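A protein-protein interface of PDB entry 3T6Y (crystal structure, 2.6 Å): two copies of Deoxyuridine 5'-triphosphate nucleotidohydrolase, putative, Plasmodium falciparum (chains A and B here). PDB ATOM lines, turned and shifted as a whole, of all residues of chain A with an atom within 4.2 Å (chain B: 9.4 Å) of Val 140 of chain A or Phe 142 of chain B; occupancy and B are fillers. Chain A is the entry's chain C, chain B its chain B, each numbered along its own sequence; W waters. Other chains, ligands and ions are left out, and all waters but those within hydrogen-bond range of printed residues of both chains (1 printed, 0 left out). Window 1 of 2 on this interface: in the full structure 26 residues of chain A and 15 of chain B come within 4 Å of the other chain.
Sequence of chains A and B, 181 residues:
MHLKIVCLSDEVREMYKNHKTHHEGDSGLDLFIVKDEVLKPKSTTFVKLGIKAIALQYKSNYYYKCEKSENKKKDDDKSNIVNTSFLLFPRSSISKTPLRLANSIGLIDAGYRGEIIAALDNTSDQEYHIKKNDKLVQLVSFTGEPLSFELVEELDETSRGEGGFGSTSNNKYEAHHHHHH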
ATOM      1  N   SER A  27     -19.026  -0.251  -8.023  1.00  0.00           N
ATOM      2  CA  SER A  27     -19.688  -1.516  -7.746  1.00  0.00           C
ATOM      3  C   SER A  27     -19.347  -2.719  -8.637  1.00  0.00           C
ATOM      4  O   SER A  27     -19.458  -3.868  -8.212  1.00  0.00           O
ATOM      5  CB  SER A  27     -21.161  -1.306  -7.815  1.00  0.00           C
ATOM      6  OG  SER A  27     -21.634  -1.402  -6.505  1.00  0.00           O
ATOM      7  N   PHE A  86     -19.241 -14.490  -5.567  1.00  0.00           N
ATOM      8  CA  PHE A  86     -19.516 -13.202  -6.179  1.00  0.00           C
ATOM      9  C   PHE A  86     -20.255 -13.426  -7.525  1.00  0.00           C
ATOM     10  O   PHE A  86     -20.580 -14.582  -7.881  1.00  0.00           O
ATOM     11  CB  PHE A  86     -18.237 -12.369  -6.265  1.00  0.00           C
ATOM     12  CG  PHE A  86     -17.176 -12.993  -7.095  1.00  0.00           C
ATOM     13  CD1 PHE A  86     -16.349 -13.973  -6.566  1.00  0.00           C
ATOM     14  CD2 PHE A  86     -17.033 -12.648  -8.456  1.00  0.00           C
ATOM     15  CE1 PHE A  86     -15.391 -14.605  -7.360  1.00  0.00           C
ATOM     16  CE2 PHE A  86     -16.079 -13.299  -9.259  1.00  0.00           C
ATOM     17  CZ  PHE A  86     -15.244 -14.277  -8.699  1.00  0.00           C
ATOM     18  N   LEU A  87     -20.550 -12.350  -8.263  1.00  0.00           N
ATOM     19  CA  LEU A  87     -21.492 -12.443  -9.373  1.00  0.00           C
ATOM     20  C   LEU A  87     -20.899 -11.908 -10.643  1.00  0.00           C
ATOM     21  O   LEU A  87     -20.118 -10.939 -10.611  1.00  0.00           O
ATOM     22  CB  LEU A  87     -22.734 -11.656  -9.060  1.00  0.00           C
ATOM     23  CG  LEU A  87     -23.504 -12.188  -7.848  1.00  0.00           C
ATOM     24  CD1 LEU A  87     -24.445 -11.144  -7.235  1.00  0.00           C
ATOM     25  CD2 LEU A  87     -24.265 -13.459  -8.172  1.00  0.00           C
ATOM     26  N   PHE A  89     -22.068 -10.125 -13.886  1.00  0.00           N
ATOM     27  CA  PHE A  89     -23.223  -9.417 -14.435  1.00  0.00           C
ATOM     28  C   PHE A  89     -22.889  -9.012 -15.875  1.00  0.00           C
ATOM     29  O   PHE A  89     -21.716  -8.771 -16.198  1.00  0.00           O
ATOM     30  CB  PHE A  89     -23.389  -8.107 -13.661  1.00  0.00           C
ATOM     31  CG  PHE A  89     -24.346  -8.154 -12.493  1.00  0.00           C
ATOM     32  CD1 PHE A  89     -24.093  -8.931 -11.380  1.00  0.00           C
ATOM     33  CD2 PHE A  89     -25.458  -7.299 -12.470  1.00  0.00           C
ATOM     34  CE1 PHE A  89     -24.969  -8.926 -10.286  1.00  0.00           C
ATOM     35  CE2 PHE A  89     -26.321  -7.281 -11.381  1.00  0.00           C
ATOM     36  CZ  PHE A  89     -26.067  -8.097 -10.282  1.00  0.00           C
ATOM     37  N   GLN A 138     -19.054  -7.845 -16.017  1.00  0.00           N
ATOM     38  CA  GLN A 138     -18.363  -7.315 -14.853  1.00  0.00           C
ATOM     39  C   GLN A 138     -18.568  -8.201 -13.639  1.00  0.00           C
ATOM     40  O   GLN A 138     -19.659  -8.806 -13.475  1.00  0.00           O
ATOM     41  CB  GLN A 138     -18.917  -5.928 -14.550  1.00  0.00           C
ATOM     42  CG  GLN A 138     -20.408  -5.937 -14.232  1.00  0.00           C
ATOM     43  CD  GLN A 138     -21.024  -4.564 -14.374  1.00  0.00           C
ATOM     44  OE1 GLN A 138     -22.209  -4.421 -14.744  1.00  0.00           O
ATOM     45  NE2 GLN A 138     -20.212  -3.524 -14.101  1.00  0.00           N
ATOM     46  N   LEU A 139     -17.555  -8.245 -12.767  1.00  0.00           N
ATOM     47  CA  LEU A 139     -17.689  -8.860 -11.425  1.00  0.00           C
ATOM     48  C   LEU A 139     -18.333  -7.900 -10.451  1.00  0.00           C
ATOM     49  O   LEU A 139     -18.073  -6.703 -10.486  1.00  0.00           O
ATOM     50  CB  LEU A 139     -16.347  -9.282 -10.881  1.00  0.00           C
ATOM     51  CG  LEU A 139     -15.611 -10.199 -11.852  1.00  0.00           C
ATOM     52  CD1 LEU A 139     -14.335 -10.724 -11.240  1.00  0.00           C
ATOM     53  CD2 LEU A 139     -16.517 -11.364 -12.277  1.00  0.00           C
ATOM     54  N   VAL A 140     -19.171  -8.414  -9.568  1.00  0.00           N
ATOM     55  CA  VAL A 140     -19.950  -7.583  -8.668  1.00  0.00           C
ATOM     56  C   VAL A 140     -20.037  -8.361  -7.360  1.00  0.00           C
ATOM     57  O   VAL A 140     -20.140  -9.601  -7.380  1.00  0.00           O
ATOM     58  CB  VAL A 140     -21.382  -7.457  -9.198  1.00  0.00           C
ATOM     59  CG1 VAL A 140     -22.255  -6.694  -8.224  1.00  0.00           C
ATOM     60  CG2 VAL A 140     -21.399  -6.861 -10.587  1.00  0.00           C
ATOM     61  N   SER A 141     -20.015  -7.650  -6.225  1.00  0.00           N
ATOM     62  CA  SER A 141     -20.172  -8.247  -4.868  1.00  0.00           C
ATOM     63  C   SER A 141     -21.640  -8.482  -4.521  1.00  0.00           C
ATOM     64  O   SER A 141     -22.486  -7.668  -4.854  1.00  0.00           O
ATOM     65  CB  SER A 141     -19.522  -7.317  -3.818  1.00  0.00           C
ATOM     66  OG  SER A 141     -19.832  -7.675  -2.470  1.00  0.00           O
ATOM     67  N   PHE A 142     -21.936  -9.565  -3.814  1.00  0.00           N
ATOM     68  CA  PHE A 142     -23.284  -9.808  -3.318  1.00  0.00           C
ATOM     69  C   PHE A 142     -23.807  -8.665  -2.453  1.00  0.00           C
ATOM     70  O   PHE A 142     -25.012  -8.570  -2.173  1.00  0.00           O
ATOM     71  CB  PHE A 142     -23.329 -11.122  -2.552  1.00  0.00           C
ATOM     72  CG  PHE A 142     -23.741 -12.310  -3.389  1.00  0.00           C
ATOM     73  CD1 PHE A 142     -25.097 -12.623  -3.575  1.00  0.00           C
ATOM     74  CD2 PHE A 142     -22.792 -13.137  -3.975  1.00  0.00           C
ATOM     75  CE1 PHE A 142     -25.493 -13.740  -4.321  1.00  0.00           C
ATOM     76  CE2 PHE A 142     -23.183 -14.249  -4.709  1.00  0.00           C
ATOM     77  CZ  PHE A 142     -24.528 -14.546  -4.906  1.00  0.00           C
ATOM     78  N   THR A 143     -22.917  -7.784  -2.036  1.00  0.00           N
ATOM     79  CA  THR A 143     -23.329  -6.656  -1.170  1.00  0.00           C
ATOM     80  C   THR A 143     -23.371  -5.340  -1.912  1.00  0.00           C
ATOM     81  O   THR A 143     -23.822  -4.348  -1.345  1.00  0.00           O
ATOM     82  CB  THR A 143     -22.394  -6.434   0.065  1.00  0.00           C
ATOM     83  OG1 THR A 143     -21.145  -5.893  -0.378  1.00  0.00           O
ATOM     84  CG2 THR A 143     -22.113  -7.719   0.824  1.00  0.00           C
ATOM     85  N   GLY A 144     -22.875  -5.303  -3.153  1.00  0.00           N
ATOM     86  CA  GLY A 144     -22.857  -4.059  -3.918  1.00  0.00           C
ATOM     87  C   GLY A 144     -21.734  -3.125  -3.502  1.00  0.00           C
ATOM     88  O   GLY A 144     -21.693  -1.993  -3.946  1.00  0.00           O
ATOM     89  N   MET B   1     -33.667  -0.726   3.000  1.00  0.00           N
ATOM     90  CA  MET B   1     -33.033   0.434   2.298  1.00  0.00           C
ATOM     91  C   MET B   1     -34.082   1.484   1.947  1.00  0.00           C
ATOM     92  O   MET B   1     -35.287   1.165   1.864  1.00  0.00           O
ATOM     93  CB  MET B   1     -32.318  -0.043   1.039  1.00  0.00           C
ATOM     94  CG  MET B   1     -32.205   0.966  -0.088  1.00  0.00           C
ATOM     95  SD  MET B   1     -31.399   0.230  -1.517  1.00  0.00           S
ATOM     96  CE  MET B   1     -32.821   0.120  -2.610  1.00  0.00           C
ATOM     97  N   SER B  27     -39.809  -6.454  -0.711  1.00  0.00           N
ATOM     98  CA  SER B  27     -38.435  -6.593  -1.159  1.00  0.00           C
ATOM     99  C   SER B  27     -38.064  -5.829  -2.390  1.00  0.00           C
ATOM    100  O   SER B  27     -36.915  -5.477  -2.567  1.00  0.00           O
ATOM    101  CB  SER B  27     -38.083  -8.046  -1.368  1.00  0.00           C
ATOM    102  OG  SER B  27     -37.044  -8.375  -0.477  1.00  0.00           O
ATOM    103  N   ALA B  55     -30.184   5.598  -3.221  1.00  0.00           N
ATOM    104  CA  ALA B  55     -30.544   4.648  -2.213  1.00  0.00           C
ATOM    105  C   ALA B  55     -29.591   4.924  -1.086  1.00  0.00           C
ATOM    106  O   ALA B  55     -28.412   5.260  -1.342  1.00  0.00           O
ATOM    107  CB  ALA B  55     -30.380   3.219  -2.727  1.00  0.00           C
ATOM    108  N   GLN B  57     -28.433   3.352   2.851  1.00  0.00           N
ATOM    109  CA  GLN B  57     -28.332   2.202   3.754  1.00  0.00           C
ATOM    110  C   GLN B  57     -27.334   2.652   4.775  1.00  0.00           C
ATOM    111  O   GLN B  57     -26.638   3.654   4.535  1.00  0.00           O
ATOM    112  CB  GLN B  57     -27.758   0.965   3.038  1.00  0.00           C
ATOM    113  CG  GLN B  57     -28.767   0.160   2.203  1.00  0.00           C
ATOM    114  CD  GLN B  57     -28.134  -0.898   1.282  1.00  0.00           C
ATOM    115  OE1 GLN B  57     -26.902  -1.025   1.213  1.00  0.00           O
ATOM    116  NE2 GLN B  57     -28.986  -1.659   0.563  1.00  0.00           N
ATOM    117  N   ASN B  83     -25.018   6.504   0.297  1.00  0.00           N
ATOM    118  CA  ASN B  83     -25.591   6.016  -0.963  1.00  0.00           C
ATOM    119  C   ASN B  83     -25.014   4.668  -1.292  1.00  0.00           C
ATOM    120  O   ASN B  83     -23.789   4.494  -1.240  1.00  0.00           O
ATOM    121  CB  ASN B  83     -25.255   6.936  -2.129  1.00  0.00           C
ATOM    122  CG  ASN B  83     -25.246   8.368  -1.733  1.00  0.00           C
ATOM    123  OD1 ASN B  83     -26.280   9.038  -1.800  1.00  0.00           O
ATOM    124  ND2 ASN B  83     -24.094   8.848  -1.254  1.00  0.00           N
ATOM    125  N   THR B  84     -25.875   3.710  -1.623  1.00  0.00           N
ATOM    126  CA  THR B  84     -25.363   2.455  -2.149  1.00  0.00           C
ATOM    127  C   THR B  84     -25.913   2.207  -3.520  1.00  0.00           C
ATOM    128  O   THR B  84     -26.923   2.782  -3.949  1.00  0.00           O
ATOM    129  CB  THR B  84     -25.706   1.235  -1.280  1.00  0.00           C
ATOM    130  OG1 THR B  84     -27.094   1.301  -0.909  1.00  0.00           O
ATOM    131  CG2 THR B  84     -24.810   1.176  -0.019  1.00  0.00           C
ATOM    132  N   SER B  85     -25.226   1.315  -4.197  1.00  0.00           N
ATOM    133  CA  SER B  85     -25.682   0.786  -5.430  1.00  0.00           C
ATOM    134  C   SER B  85     -26.979   0.048  -5.124  1.00  0.00           C
ATOM    135  O   SER B  85     -27.189  -0.355  -3.975  1.00  0.00           O
ATOM    136  CB  SER B  85     -24.622  -0.161  -5.939  1.00  0.00           C
ATOM    137  OG  SER B  85     -23.428   0.586  -6.171  1.00  0.00           O
ATOM    138  N   PHE B  86     -27.861  -0.036  -6.134  1.00  0.00           N
ATOM    139  CA  PHE B  86     -29.038  -0.867  -6.080  1.00  0.00           C
ATOM    140  C   PHE B  86     -29.259  -1.602  -7.451  1.00  0.00           C
ATOM    141  O   PHE B  86     -28.404  -1.528  -8.365  1.00  0.00           O
ATOM    142  CB  PHE B  86     -30.242  -0.087  -5.581  1.00  0.00           C
ATOM    143  CG  PHE B  86     -30.515   1.201  -6.354  1.00  0.00           C
ATOM    144  CD1 PHE B  86     -29.747   2.353  -6.143  1.00  0.00           C
ATOM    145  CD2 PHE B  86     -31.572   1.280  -7.256  1.00  0.00           C
ATOM    146  CE1 PHE B  86     -30.023   3.540  -6.808  1.00  0.00           C
ATOM    147  CE2 PHE B  86     -31.822   2.443  -7.959  1.00  0.00           C
ATOM    148  CZ  PHE B  86     -31.039   3.581  -7.731  1.00  0.00           C
ATOM    149  N   LEU B  87     -30.362  -2.341  -7.578  1.00  0.00           N
ATOM    150  CA  LEU B  87     -30.514  -3.242  -8.694  1.00  0.00           C
ATOM    151  C   LEU B  87     -31.795  -2.985  -9.380  1.00  0.00           C
ATOM    152  O   LEU B  87     -32.751  -2.564  -8.741  1.00  0.00           O
ATOM    153  CB  LEU B  87     -30.509  -4.664  -8.216  1.00  0.00           C
ATOM    154  CG  LEU B  87     -29.183  -5.019  -7.578  1.00  0.00           C
ATOM    155  CD1 LEU B  87     -29.381  -6.325  -6.830  1.00  0.00           C
ATOM    156  CD2 LEU B  87     -28.084  -5.136  -8.632  1.00  0.00           C
ATOM    157  N   LEU B  88     -31.835  -3.215 -10.687  1.00  0.00           N
ATOM    158  CA  LEU B  88     -33.110  -3.112 -11.401  1.00  0.00           C
ATOM    159  C   LEU B  88     -33.501  -4.507 -11.864  1.00  0.00           C
ATOM    160  O   LEU B  88     -32.829  -5.073 -12.755  1.00  0.00           O
ATOM    161  CB  LEU B  88     -32.967  -2.135 -12.568  1.00  0.00           C
ATOM    162  CG  LEU B  88     -34.199  -2.021 -13.461  1.00  0.00           C
ATOM    163  CD1 LEU B  88     -35.234  -1.071 -12.860  1.00  0.00           C
ATOM    164  CD2 LEU B  88     -33.797  -1.586 -14.876  1.00  0.00           C
ATOM    165  N   PHE B  89     -34.502  -5.098 -11.222  1.00  0.00           N
ATOM    166  CA  PHE B  89     -34.978  -6.401 -11.642  1.00  0.00           C
ATOM    167  C   PHE B  89     -36.227  -6.306 -12.515  1.00  0.00           C
ATOM    168  O   PHE B  89     -37.075  -5.424 -12.297  1.00  0.00           O
ATOM    169  CB  PHE B  89     -35.469  -7.224 -10.469  1.00  0.00           C
ATOM    170  CG  PHE B  89     -34.408  -7.937  -9.705  1.00  0.00           C
ATOM    171  CD1 PHE B  89     -33.338  -7.255  -9.163  1.00  0.00           C
ATOM    172  CD2 PHE B  89     -34.552  -9.282  -9.426  1.00  0.00           C
ATOM    173  CE1 PHE B  89     -32.377  -7.922  -8.406  1.00  0.00           C
ATOM    174  CE2 PHE B  89     -33.599  -9.953  -8.666  1.00  0.00           C
ATOM    175  CZ  PHE B  89     -32.502  -9.265  -8.158  1.00  0.00           C
ATOM    176  N   ILE B 105     -30.268  -7.951 -15.279  1.00  0.00           N
ATOM    177  CA  ILE B 105     -30.508  -7.249 -14.038  1.00  0.00           C
ATOM    178  C   ILE B 105     -29.719  -5.936 -14.090  1.00  0.00           C
ATOM    179  O   ILE B 105     -28.511  -5.962 -14.355  1.00  0.00           O
ATOM    180  CB  ILE B 105     -29.964  -8.054 -12.846  1.00  0.00           C
ATOM    181  CG1 ILE B 105     -30.727  -9.375 -12.628  1.00  0.00           C
ATOM    182  CG2 ILE B 105     -30.035  -7.218 -11.583  1.00  0.00           C
ATOM    183  CD1 ILE B 105     -32.214  -9.253 -12.384  1.00  0.00           C
ATOM    184  N   GLY B 106     -30.363  -4.795 -13.877  1.00  0.00           N
ATOM    185  CA  GLY B 106     -29.647  -3.542 -14.076  1.00  0.00           C
ATOM    186  C   GLY B 106     -28.851  -3.188 -12.830  1.00  0.00           C
ATOM    187  O   GLY B 106     -29.345  -3.315 -11.708  1.00  0.00           O
ATOM    188  N   LEU B 107     -27.620  -2.737 -12.985  1.00  0.00           N
ATOM    189  CA  LEU B 107     -26.889  -2.313 -11.802  1.00  0.00           C
ATOM    190  C   LEU B 107     -26.820  -0.782 -11.781  1.00  0.00           C
ATOM    191  O   LEU B 107     -26.169  -0.199 -12.633  1.00  0.00           O
ATOM    192  CB  LEU B 107     -25.493  -2.917 -11.808  1.00  0.00           C
ATOM    193  CG  LEU B 107     -24.479  -2.362 -10.814  1.00  0.00           C
ATOM    194  CD1 LEU B 107     -24.922  -2.737  -9.420  1.00  0.00           C
ATOM    195  CD2 LEU B 107     -23.085  -2.895 -11.077  1.00  0.00           C
ATOM    196  N   ILE B 108     -27.524  -0.126 -10.854  1.00  0.00           N
ATOM    197  CA  ILE B 108     -27.406   1.308 -10.738  1.00  0.00           C
ATOM    198  C   ILE B 108     -26.299   1.630  -9.700  1.00  0.00           C
ATOM    199  O   ILE B 108     -26.434   1.287  -8.510  1.00  0.00           O
ATOM    200  CB  ILE B 108     -28.728   1.906 -10.258  1.00  0.00           C
ATOM    201  CG1 ILE B 108     -29.927   1.360 -11.028  1.00  0.00           C
ATOM    202  CG2 ILE B 108     -28.678   3.435 -10.261  1.00  0.00           C
ATOM    203  CD1 ILE B 108     -29.930   1.667 -12.503  1.00  0.00           C
ATOM    204  N   ASP B 109     -25.217   2.288 -10.103  1.00  0.00           N
ATOM    205  CA  ASP B 109     -24.137   2.579  -9.154  1.00  0.00           C
ATOM    206  C   ASP B 109     -24.443   3.660  -8.096  1.00  0.00           C
ATOM    207  O   ASP B 109     -25.270   4.554  -8.303  1.00  0.00           O
ATOM    208  CB  ASP B 109     -22.858   2.936  -9.898  1.00  0.00           C
ATOM    209  CG  ASP B 109     -21.615   2.521  -9.136  1.00  0.00           C
ATOM    210  OD1 ASP B 109     -21.330   1.295  -9.107  1.00  0.00           O
ATOM    211  OD2 ASP B 109     -20.921   3.414  -8.579  1.00  0.00           O
ATOM    212  N   ALA B 110     -23.766   3.571  -6.957  1.00  0.00           N
ATOM    213  CA  ALA B 110     -23.858   4.616  -5.911  1.00  0.00           C
ATOM    214  C   ALA B 110     -23.727   6.042  -6.462  1.00  0.00           C
ATOM    215  O   ALA B 110     -24.506   6.928  -6.069  1.00  0.00           O
ATOM    216  CB  ALA B 110     -22.843   4.381  -4.788  1.00  0.00           C
ATOM    217  N   LEU B 139     -37.225  -1.955  -8.333  1.00  0.00           N
ATOM    218  CA  LEU B 139     -35.947  -1.585  -7.723  1.00  0.00           C
ATOM    219  C   LEU B 139     -35.805  -2.513  -6.542  1.00  0.00           C
ATOM    220  O   LEU B 139     -36.782  -2.764  -5.855  1.00  0.00           O
ATOM    221  CB  LEU B 139     -35.957  -0.140  -7.269  1.00  0.00           C
ATOM    222  CG  LEU B 139     -35.784   0.824  -8.430  1.00  0.00           C
ATOM    223  CD1 LEU B 139     -35.922   2.243  -7.918  1.00  0.00           C
ATOM    224  CD2 LEU B 139     -34.428   0.671  -9.157  1.00  0.00           C
ATOM    225  N   VAL B 140     -34.621  -3.078  -6.366  1.00  0.00           N
ATOM    226  CA  VAL B 140     -34.328  -4.093  -5.351  1.00  0.00           C
ATOM    227  C   VAL B 140     -32.968  -3.693  -4.733  1.00  0.00           C
ATOM    228  O   VAL B 140     -32.118  -3.036  -5.347  1.00  0.00           O
ATOM    229  CB  VAL B 140     -34.242  -5.484  -6.016  1.00  0.00           C
ATOM    230  CG1 VAL B 140     -33.833  -6.585  -5.039  1.00  0.00           C
ATOM    231  CG2 VAL B 140     -35.562  -5.830  -6.674  1.00  0.00           C
ATOM    232  N   SER B 141     -32.778  -4.021  -3.479  1.00  0.00           N
ATOM    233  CA  SER B 141     -31.547  -3.663  -2.817  1.00  0.00           C
ATOM    234  C   SER B 141     -30.661  -4.880  -2.800  1.00  0.00           C
ATOM    235  O   SER B 141     -31.126  -6.027  -2.736  1.00  0.00           O
ATOM    236  CB  SER B 141     -31.880  -3.218  -1.388  1.00  0.00           C
ATOM    237  OG  SER B 141     -30.909  -3.609  -0.433  1.00  0.00           O
ATOM    238  N   PHE B 142     -29.370  -4.621  -2.743  1.00  0.00           N
ATOM    239  CA  PHE B 142     -28.392  -5.689  -2.627  1.00  0.00           C
ATOM    240  C   PHE B 142     -28.576  -6.728  -1.534  1.00  0.00           C
ATOM    241  O   PHE B 142     -28.092  -7.854  -1.635  1.00  0.00           O
ATOM    242  CB  PHE B 142     -27.010  -5.088  -2.608  1.00  0.00           C
ATOM    243  CG  PHE B 142     -26.400  -5.036  -3.963  1.00  0.00           C
ATOM    244  CD1 PHE B 142     -25.795  -6.169  -4.509  1.00  0.00           C
ATOM    245  CD2 PHE B 142     -26.464  -3.888  -4.723  1.00  0.00           C
ATOM    246  CE1 PHE B 142     -25.216  -6.125  -5.780  1.00  0.00           C
ATOM    247  CE2 PHE B 142     -25.887  -3.849  -5.997  1.00  0.00           C
ATOM    248  CZ  PHE B 142     -25.269  -4.959  -6.533  1.00  0.00           C
ATOM    249  N   THR B 143     -29.310  -6.379  -0.513  1.00  0.00           N
ATOM    250  CA  THR B 143     -29.440  -7.274   0.628  1.00  0.00           C
ATOM    251  C   THR B 143     -30.813  -7.924   0.688  1.00  0.00           C
ATOM    252  O   THR B 143     -31.087  -8.796   1.546  1.00  0.00           O
ATOM    253  CB  THR B 143     -29.155  -6.513   1.963  1.00  0.00           C
ATOM    254  OG1 THR B 143     -29.965  -5.310   1.995  1.00  0.00           O
ATOM    255  CG2 THR B 143     -27.610  -6.165   2.105  1.00  0.00           C
ATOM    256  N   GLY B 144     -31.693  -7.502  -0.205  1.00  0.00           N
ATOM    257  CA  GLY B 144     -33.032  -8.050  -0.171  1.00  0.00           C
ATOM    258  C   GLY B 144     -33.922  -7.439   0.896  1.00  0.00           C
ATOM    259  O   GLY B 144     -35.098  -7.822   1.016  1.00  0.00           O
ATOM    260  N   GLU B 145     -33.379  -6.473   1.638  1.00  0.00           N
ATOM    261  CA  GLU B 145     -34.113  -5.798   2.692  1.00  0.00           C
ATOM    262  C   GLU B 145     -35.281  -4.994   2.138  1.00  0.00           C
ATOM    263  O   GLU B 145     -35.196  -4.520   0.999  1.00  0.00           O
ATOM    264  CB  GLU B 145     -33.180  -4.874   3.511  1.00  0.00           C
ATOM    265  CG  GLU B 145     -32.487  -3.724   2.784  1.00  0.00           C
ATOM    266  CD  GLU B 145     -31.217  -3.306   3.536  1.00  0.00           C
ATOM    267  OE1 GLU B 145     -30.719  -4.177   4.297  1.00  0.00           O
ATOM    268  OE2 GLU B 145     -30.698  -2.149   3.423  1.00  0.00           O
ATOM    269  N   PRO B 146     -36.364  -4.826   2.949  1.00  0.00           N
ATOM    270  CA  PRO B 146     -37.542  -4.000   2.652  1.00  0.00           C
ATOM    271  C   PRO B 146     -37.174  -2.584   2.217  1.00  0.00           C
ATOM    272  O   PRO B 146     -36.241  -1.965   2.756  1.00  0.00           O
ATOM    273  CB  PRO B 146     -38.267  -3.956   3.991  1.00  0.00           C
ATOM    274  CG  PRO B 146     -37.923  -5.258   4.639  1.00  0.00           C
ATOM    275  CD  PRO B 146     -36.496  -5.493   4.265  1.00  0.00           C
ATOM    276  N   LEU B 147     -37.899  -2.076   1.230  1.00  0.00           N
ATOM    277  CA  LEU B 147     -37.531  -0.813   0.618  1.00  0.00           C
ATOM    278  C   LEU B 147     -38.498   0.228   1.070  1.00  0.00           C
ATOM    279  O   LEU B 147     -39.631  -0.128   1.395  1.00  0.00           O
ATOM    280  CB  LEU B 147     -37.604  -0.937  -0.890  1.00  0.00           C
ATOM    281  CG  LEU B 147     -36.231  -0.909  -1.534  1.00  0.00           C
ATOM    282  CD1 LEU B 147     -35.433  -2.129  -1.090  1.00  0.00           C
ATOM    283  CD2 LEU B 147     -36.426  -0.873  -3.038  1.00  0.00           C
HETATM  284  O   HOH W   1     -27.393  -9.698  -3.729  1.00  0.00           O
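Water W1 lies within hydrogen-bond range of O of Phe 142 of chain B (2.9 Å) and O of Phe 142 of chain A (3.1 Å).
Among the printed residues, pairs that only touch across the chains: Phe 89 of chain A with Leu 87 of chain B (3.9 Å), Phe 89 of chain A with Ile 105 of chain B (3.7 Å), Val 140 of chain A with Phe 142 of chain B (3.9 Å), Ser 141 of chain A with Phe 142 of chain B (3.3 Å), Thr 143 of chain A with Phe 142 of chain B (3.5 Å), Gly 144 of chain A with Ser 85 of chain B (3.8 Å) and Gly 144 of chain A with Phe 142 of chain B (3.3 Å).
The side-chain hydroxyl (OG) of Ser 85 of chain B is in hydrogen-bond range of the side-chain hydroxyl (OG) of Ser 27 of chain A, 2.7 Å away.
OD1 of Asp 109 of chain B lies close to N of Ser 27 of chain A, 3.0 Å away.
The backbone carbonyl oxygen (O) of Phe 142 of chain B lies close to the backbone carbonyl oxygen (O) of Phe 142 of chain A, at 3.2 Å.
Hydrophobic or aromatic side chains of chain B that line the printed part of chain A: Leu 87, Ile 105 and Phe 142.
Along chain A the printed residues that touch a printed residue of chain B span positions 27 to 144.
Among the printed residues, 10 pairs touch across the chains.
Among the printed residues, no Asp or Glu carboxylate lies within 4 Å of a Lys or Arg side-chain nitrogen of the other chain.
Printed residues of chain B within 4 Å of Ser 27 of chain A: Ser 85 (2.7 Å) and Asp 109 (2.9 Å).
Of the printed residues of chain B, Phe 89 of chain A touches Leu 87 (3.9 Å) and Ile 105 (3.7 Å).
Of the printed residues of chain B, Thr 143 of chain A touches Phe 142.
Gly 144 of chain A touches just these residues of chain B: Ser 85 and Phe 142.
Thr 84 of chain B touches none of the printed residues of chain A.
Printed residues of chain A within 4 Å of Ile 105 of chain B: Phe 89.
Of chain A, only Val 140 (3.9 Å), Ser 141 (3.3 Å), Phe 142 (3.2 Å), Thr 143 (3.5 Å) and Gly 144 (3.3 Å) come within 4 Å of Phe 142 of chain B.
Pro 146 of chain B touches none of the printed residues of chain A.
The nearest residue of chain B that does not touch Val 140 of chain A is Leu 107 of chain B (4.3 Å).
Phe 89 of chain A touches Leu 87 of chain B, but with the chains exchanged Leu 87 of chain A does not touch Phe 89 of chain B (8.3 Å).
Val 140 of chain A touches Phe 142 of chain B, but with the chains exchanged Phe 142 of chain A does not touch Val 140 of chain B (9.5 Å).
Ser 141 of chain A touches Phe 142 of chain B, but with the chains exchanged Phe 142 of chain A does not touch Ser 141 of chain B (6.6 Å).
Thr 143 of chain A touches Phe 142 of chain B, but with the chains exchanged Phe 142 of chain A does not touch Thr 143 of chain B (5.1 Å).
Of the 10 pairs that touch across the chains among the printed residues, 1 has its exchanged pair printed and touching as well.
The side-chain hydroxyl of Ser 85 of chain B lies within hydrogen-bond range of the backbone NH of Ala 110 of chain B (3.1 Å).
O of Val 140 of chain B lies within hydrogen-bond range of N of Leu 87 of chain B (2.9 Å).
OG of Ser 27 of chain A lies within hydrogen-bond range of O of Gly 144 of chain A.
O of Leu 87 of chain A sits at hydrogen-bond distance from N of Val 140 of chain A (2.9 Å).
O of Gln 138 of chain A lies within hydrogen-bond range of N of Phe 89 of chain A, 2.8 Å away.
OG1 of Thr 143 of chain A is in hydrogen-bond range of OG of Ser 141 of chain A, 3.0 Å away.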
